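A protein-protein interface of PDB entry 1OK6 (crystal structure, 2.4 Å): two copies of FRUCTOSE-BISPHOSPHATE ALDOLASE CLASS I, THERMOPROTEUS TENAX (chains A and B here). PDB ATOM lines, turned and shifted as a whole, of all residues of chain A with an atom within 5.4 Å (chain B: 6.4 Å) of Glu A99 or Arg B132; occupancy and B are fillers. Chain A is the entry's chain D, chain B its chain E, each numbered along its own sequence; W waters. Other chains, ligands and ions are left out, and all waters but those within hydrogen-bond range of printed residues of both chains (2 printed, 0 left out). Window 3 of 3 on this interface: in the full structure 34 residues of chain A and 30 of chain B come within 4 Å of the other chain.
NH1 of Arg B132 lies within salt-bridge range of OE1 of Glu A99 (3.5 Å). NH2 of Arg B132 is in hydrogen-bond range of OG of Ser A97 (3.4 Å). OE1 of Glu A100 lies within salt-bridge range of NE of Arg B132 (3.7 Å).
The guanidinium group (NH2) of Arg A62 is in salt-bridge range of the side-chain carboxylate (OE1) of Glu A100, at 3.6 Å. The side-chain hydroxyl (OG) of Ser A97 lies within hydrogen-bond range of the side-chain carboxylate (OE1) of Glu A100 (2.7 Å). O of Glu A100 sits at hydrogen-bond distance from OG of Ser A103 (3.1 Å).
Among the printed residues, pairs that only touch across the chains: Arg A62 with Lys B131 (3.3 Å).
Glu A99 touches just one residue of chain B: Arg B132 (3.5 Å). Arg B132 touches just these residues of chain A: Ser A97, Glu A99 and Glu A100. Printed residues of chain A within 4 Å of Lys B131: Arg A62. Printed residues of chain B within 4 Å of Glu A100: Arg B132 (3.2 Å). Of the printed residues of chain B, Ser A97 touches Arg B132. The nearest printed residue of chain B that does not touch Glu A99 is Lys B136 (9.0 Å). The nearest printed residue of chain A that does not touch Lys B131 is Glu A100 (4.8 Å).
Of the 11 printed residues of chain B, 2 touch a printed residue of chain A. Printed residues of chain B that touch a printed residue of chain A: Lys B131 and Arg B132. Among the printed residues, 4 pairs touch across the chains. Among the printed residues, Asp or Glu carboxylates within 4 Å of a Lys or Arg side-chain nitrogen of the other chain: Glu A99 with Arg B132 (3.5 Å) and Glu A100 with Arg B132 (3.7 Å).
Position printed for both chains: 137. Of the 4 pairs that touch across the chains among the printed residues, none has its exchanged pair printed and touching as well.
Water W2 lies within hydrogen-bond range of O of Ala B128 (2.6 Å), OE1 of Glu A100 (2.7 Å) and NH1 of Arg A62 (3.1 Å). Water W1 lies within hydrogen-bond range of OE1 of Glu A99 and NH2 of Arg B132.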
ATOM      1  N   ARG A  62      12.429   6.192  34.274  1.00  0.00           N
ATOM      2  CA  ARG A  62      12.317   6.507  32.867  1.00  0.00           C
ATOM      3  C   ARG A  62      11.123   7.420  32.489  1.00  0.00           C
ATOM      4  O   ARG A  62      11.275   8.314  31.656  1.00  0.00           O
ATOM      5  CB  ARG A  62      12.266   5.232  32.047  1.00  0.00           C
ATOM      6  CG  ARG A  62      11.771   5.550  30.680  1.00  0.00           C
ATOM      7  CD  ARG A  62      10.483   4.871  30.313  1.00  0.00           C
ATOM      8  NE  ARG A  62      10.737   4.454  28.969  1.00  0.00           N
ATOM      9  CZ  ARG A  62      11.002   3.248  28.579  1.00  0.00           C
ATOM     10  NH1 ARG A  62      10.946   2.202  29.400  1.00  0.00           N
ATOM     11  NH2 ARG A  62      11.249   3.102  27.295  1.00  0.00           N
ATOM     12  N   SER A  97      15.533   0.279  29.871  1.00  0.00           N
ATOM     13  CA  SER A  97      16.777  -0.313  29.398  1.00  0.00           C
ATOM     14  C   SER A  97      17.892   0.714  29.332  1.00  0.00           C
ATOM     15  O   SER A  97      17.632   1.946  29.301  1.00  0.00           O
ATOM     16  CB  SER A  97      16.561  -0.919  28.015  1.00  0.00           C
ATOM     17  OG  SER A  97      16.346   0.104  27.069  1.00  0.00           O
ATOM     18  N   VAL A  98      19.137   0.214  29.323  1.00  0.00           N
ATOM     19  CA  VAL A  98      20.294   1.068  29.156  1.00  0.00           C
ATOM     20  C   VAL A  98      20.201   1.813  27.833  1.00  0.00           C
ATOM     21  O   VAL A  98      20.389   3.018  27.807  1.00  0.00           O
ATOM     22  CB  VAL A  98      21.600   0.278  29.256  1.00  0.00           C
ATOM     23  CG1 VAL A  98      22.803   1.181  29.018  1.00  0.00           C
ATOM     24  CG2 VAL A  98      21.714  -0.380  30.640  1.00  0.00           C
ATOM     25  N   GLU A  99      19.880   1.109  26.745  1.00  0.00           N
ATOM     26  CA  GLU A  99      19.784   1.729  25.422  1.00  0.00           C
ATOM     27  C   GLU A  99      18.817   2.917  25.383  1.00  0.00           C
ATOM     28  O   GLU A  99      19.110   3.946  24.767  1.00  0.00           O
ATOM     29  CB  GLU A  99      19.373   0.705  24.369  1.00  0.00           C
ATOM     30  CG  GLU A  99      19.136   1.313  22.990  1.00  0.00           C
ATOM     31  CD  GLU A  99      19.110   0.282  21.873  1.00  0.00           C
ATOM     32  OE1 GLU A  99      19.328  -0.932  22.141  1.00  0.00           O
ATOM     33  OE2 GLU A  99      18.866   0.699  20.719  1.00  0.00           O
ATOM     34  N   GLU A 100      17.672   2.783  26.040  1.00  0.00           N
ATOM     35  CA  GLU A 100      16.704   3.886  26.100  1.00  0.00           C
ATOM     36  C   GLU A 100      17.199   5.021  26.996  1.00  0.00           C
ATOM     37  O   GLU A 100      17.001   6.209  26.672  1.00  0.00           O
ATOM     38  CB  GLU A 100      15.305   3.386  26.490  1.00  0.00           C
ATOM     39  CG  GLU A 100      14.759   2.401  25.472  1.00  0.00           C
ATOM     40  CD  GLU A 100      13.542   1.643  25.958  1.00  0.00           C
ATOM     41  OE1 GLU A 100      13.712   0.608  26.623  1.00  0.00           O
ATOM     42  OE2 GLU A 100      12.402   2.075  25.637  1.00  0.00           O
ATOM     43  N   ALA A 101      17.857   4.661  28.094  1.00  0.00           N
ATOM     44  CA  ALA A 101      18.471   5.642  28.982  1.00  0.00           C
ATOM     45  C   ALA A 101      19.459   6.515  28.225  1.00  0.00           C
ATOM     46  O   ALA A 101      19.474   7.757  28.394  1.00  0.00           O
ATOM     47  CB  ALA A 101      19.156   4.967  30.125  1.00  0.00           C
ATOM     48  N   VAL A 102      20.260   5.874  27.364  1.00  0.00           N
ATOM     49  CA  VAL A 102      21.230   6.590  26.547  1.00  0.00           C
ATOM     50  C   VAL A 102      20.540   7.642  25.713  1.00  0.00           C
ATOM     51  O   VAL A 102      20.955   8.789  25.713  1.00  0.00           O
ATOM     52  CB  VAL A 102      22.048   5.636  25.634  1.00  0.00           C
ATOM     53  CG1 VAL A 102      22.775   6.410  24.524  1.00  0.00           C
ATOM     54  CG2 VAL A 102      23.060   4.852  26.465  1.00  0.00           C
ATOM     55  N   SER A 103      19.459   7.250  25.046  1.00  0.00           N
ATOM     56  CA  SER A 103      18.752   8.134  24.135  1.00  0.00           C
ATOM     57  C   SER A 103      17.993   9.234  24.883  1.00  0.00           C
ATOM     58  O   SER A 103      17.636  10.243  24.281  1.00  0.00           O
ATOM     59  CB  SER A 103      17.824   7.333  23.193  1.00  0.00           C
ATOM     60  OG  SER A 103      16.518   7.192  23.738  1.00  0.00           O
ATOM     61  N   PHE A 137      27.171   0.476  26.255  1.00  0.00           N
ATOM     62  CA  PHE A 137      26.797   1.857  25.989  1.00  0.00           C
ATOM     63  C   PHE A 137      27.695   2.863  26.729  1.00  0.00           C
ATOM     64  O   PHE A 137      27.471   4.071  26.653  1.00  0.00           O
ATOM     65  CB  PHE A 137      25.299   2.089  26.268  1.00  0.00           C
ATOM     66  CG  PHE A 137      24.389   1.403  25.268  1.00  0.00           C
ATOM     67  CD1 PHE A 137      24.057   2.027  24.057  1.00  0.00           C
ATOM     68  CD2 PHE A 137      23.895   0.128  25.521  1.00  0.00           C
ATOM     69  CE1 PHE A 137      23.218   1.383  23.097  1.00  0.00           C
ATOM     70  CE2 PHE A 137      23.068  -0.538  24.579  1.00  0.00           C
ATOM     71  CZ  PHE A 137      22.724   0.102  23.353  1.00  0.00           C
ATOM     72  N   LEU B 127       5.579  -4.432  30.745  1.00  0.00           N
ATOM     73  CA  LEU B 127       5.446  -3.021  30.395  1.00  0.00           C
ATOM     74  C   LEU B 127       6.721  -2.410  29.777  1.00  0.00           C
ATOM     75  O   LEU B 127       6.645  -1.564  28.859  1.00  0.00           O
ATOM     76  CB  LEU B 127       4.955  -2.193  31.583  1.00  0.00           C
ATOM     77  CG  LEU B 127       4.425  -0.785  31.276  1.00  0.00           C
ATOM     78  CD1 LEU B 127       3.357  -0.828  30.169  1.00  0.00           C
ATOM     79  CD2 LEU B 127       3.872  -0.105  32.518  1.00  0.00           C
ATOM     80  N   ALA B 128       7.879  -2.836  30.263  1.00  0.00           N
ATOM     81  CA  ALA B 128       9.141  -2.334  29.720  1.00  0.00           C
ATOM     82  C   ALA B 128       9.208  -2.584  28.204  1.00  0.00           C
ATOM     83  O   ALA B 128       9.550  -1.694  27.438  1.00  0.00           O
ATOM     84  CB  ALA B 128      10.296  -2.997  30.406  1.00  0.00           C
ATOM     85  N   ARG B 129       8.867  -3.804  27.787  1.00  0.00           N
ATOM     86  CA  ARG B 129       8.868  -4.177  26.373  1.00  0.00           C
ATOM     87  C   ARG B 129       7.817  -3.385  25.600  1.00  0.00           C
ATOM     88  O   ARG B 129       8.104  -2.863  24.530  1.00  0.00           O
ATOM     89  CB  ARG B 129       8.647  -5.697  26.165  1.00  0.00           C
ATOM     90  CG  ARG B 129       9.828  -6.562  26.644  1.00  0.00           C
ATOM     91  CD  ARG B 129       9.629  -8.094  26.473  1.00  0.00           C
ATOM     92  NE  ARG B 129       9.547  -8.762  27.775  1.00  0.00           N
ATOM     93  CZ  ARG B 129       8.481  -9.437  28.220  1.00  0.00           C
ATOM     94  NH1 ARG B 129       7.383  -9.560  27.461  1.00  0.00           N
ATOM     95  NH2 ARG B 129       8.519  -9.991  29.434  1.00  0.00           N
ATOM     96  N   ILE B 130       6.624  -3.291  26.155  1.00  0.00           N
ATOM     97  CA  ILE B 130       5.531  -2.592  25.500  1.00  0.00           C
ATOM     98  C   ILE B 130       5.789  -1.080  25.342  1.00  0.00           C
ATOM     99  O   ILE B 130       5.551  -0.520  24.271  1.00  0.00           O
ATOM    100  CB  ILE B 130       4.217  -2.896  26.229  1.00  0.00           C
ATOM    101  CG1 ILE B 130       3.848  -4.360  25.962  1.00  0.00           C
ATOM    102  CG2 ILE B 130       3.109  -1.947  25.773  1.00  0.00           C
ATOM    103  CD1 ILE B 130       2.777  -4.901  26.835  1.00  0.00           C
ATOM    104  N   LYS B 131       6.305  -0.443  26.396  1.00  0.00           N
ATOM    105  CA  LYS B 131       6.692   0.958  26.339  1.00  0.00           C
ATOM    106  C   LYS B 131       7.736   1.193  25.244  1.00  0.00           C
ATOM    107  O   LYS B 131       7.626   2.126  24.450  1.00  0.00           O
ATOM    108  CB  LYS B 131       7.251   1.398  27.694  1.00  0.00           C
ATOM    109  CG  LYS B 131       7.807   2.796  27.738  1.00  0.00           C
ATOM    110  CD  LYS B 131       6.778   3.865  27.340  1.00  0.00           C
ATOM    111  CE  LYS B 131       7.485   5.179  27.178  1.00  0.00           C
ATOM    112  NZ  LYS B 131       6.518   6.307  27.049  1.00  0.00           N
ATOM    113  N   ARG B 132       8.751   0.333  25.198  1.00  0.00           N
ATOM    114  CA  ARG B 132       9.770   0.428  24.177  1.00  0.00           C
ATOM    115  C   ARG B 132       9.140   0.310  22.783  1.00  0.00           C
ATOM    116  O   ARG B 132       9.439   1.118  21.897  1.00  0.00           O
ATOM    117  CB  ARG B 132      10.832  -0.649  24.374  1.00  0.00           C
ATOM    118  CG  ARG B 132      12.096  -0.400  23.563  1.00  0.00           C
ATOM    119  CD  ARG B 132      12.873  -1.637  23.113  1.00  0.00           C
ATOM    120  NE  ARG B 132      13.997  -1.974  23.963  1.00  0.00           N
ATOM    121  CZ  ARG B 132      15.325  -1.864  23.755  1.00  0.00           C
ATOM    122  NH1 ARG B 132      15.900  -1.355  22.659  1.00  0.00           N
ATOM    123  NH2 ARG B 132      16.094  -2.300  24.736  1.00  0.00           N
ATOM    124  N   ASP B 133       8.290  -0.695  22.586  1.00  0.00           N
ATOM    125  CA  ASP B 133       7.545  -0.850  21.328  1.00  0.00           C
ATOM    126  C   ASP B 133       6.660   0.350  20.989  1.00  0.00           C
ATOM    127  O   ASP B 133       6.620   0.756  19.835  1.00  0.00           O
ATOM    128  CB  ASP B 133       6.686  -2.104  21.349  1.00  0.00           C
ATOM    129  CG  ASP B 133       7.491  -3.358  21.209  1.00  0.00           C
ATOM    130  OD1 ASP B 133       8.684  -3.273  20.807  1.00  0.00           O
ATOM    131  OD2 ASP B 133       7.008  -4.485  21.476  1.00  0.00           O
ATOM    132  N   ALA B 134       5.981   0.913  21.989  1.00  0.00           N
ATOM    133  CA  ALA B 134       5.102   2.059  21.772  1.00  0.00           C
ATOM    134  C   ALA B 134       5.884   3.225  21.207  1.00  0.00           C
ATOM    135  O   ALA B 134       5.464   3.823  20.230  1.00  0.00           O
ATOM    136  CB  ALA B 134       4.390   2.449  23.038  1.00  0.00           C
ATOM    137  N   VAL B 135       7.035   3.522  21.806  1.00  0.00           N
ATOM    138  CA  VAL B 135       7.918   4.573  21.321  1.00  0.00           C
ATOM    139  C   VAL B 135       8.364   4.231  19.895  1.00  0.00           C
ATOM    140  O   VAL B 135       8.303   5.060  18.995  1.00  0.00           O
ATOM    141  CB  VAL B 135       9.168   4.791  22.267  1.00  0.00           C
ATOM    142  CG1 VAL B 135      10.228   5.705  21.615  1.00  0.00           C
ATOM    143  CG2 VAL B 135       8.757   5.338  23.638  1.00  0.00           C
ATOM    144  N   LYS B 136       8.805   3.000  19.693  1.00  0.00           N
ATOM    145  CA  LYS B 136       9.299   2.561  18.392  1.00  0.00           C
ATOM    146  C   LYS B 136       8.253   2.741  17.285  1.00  0.00           C
ATOM    147  O   LYS B 136       8.583   3.225  16.197  1.00  0.00           O
ATOM    148  CB  LYS B 136       9.748   1.112  18.484  1.00  0.00           C
ATOM    149  CG  LYS B 136      10.073   0.437  17.144  1.00  0.00           C
ATOM    150  CD  LYS B 136      10.646  -0.953  17.405  1.00  0.00           C
ATOM    151  CE  LYS B 136      10.766  -1.746  16.114  1.00  0.00           C
ATOM    152  NZ  LYS B 136      11.105  -3.156  16.386  1.00  0.00           N
ATOM    153  N   PHE B 137       7.003   2.373  17.564  1.00  0.00           N
ATOM    154  CA  PHE B 137       5.937   2.498  16.574  1.00  0.00           C
ATOM    155  C   PHE B 137       5.188   3.852  16.637  1.00  0.00           C
ATOM    156  O   PHE B 137       4.224   4.072  15.902  1.00  0.00           O
ATOM    157  CB  PHE B 137       4.983   1.289  16.664  1.00  0.00           C
ATOM    158  CG  PHE B 137       5.618  -0.015  16.187  1.00  0.00           C
ATOM    159  CD1 PHE B 137       5.605  -0.363  14.826  1.00  0.00           C
ATOM    160  CD2 PHE B 137       6.264  -0.863  17.089  1.00  0.00           C
ATOM    161  CE1 PHE B 137       6.205  -1.559  14.369  1.00  0.00           C
ATOM    162  CE2 PHE B 137       6.886  -2.054  16.659  1.00  0.00           C
ATOM    163  CZ  PHE B 137       6.848  -2.408  15.285  1.00  0.00           C
HETATM  164  O   HOH W   1      19.308  -2.803  24.218  1.00  0.00           O
HETATM  165  O   HOH W   2      11.754  -0.510  28.176  1.00  0.00           O
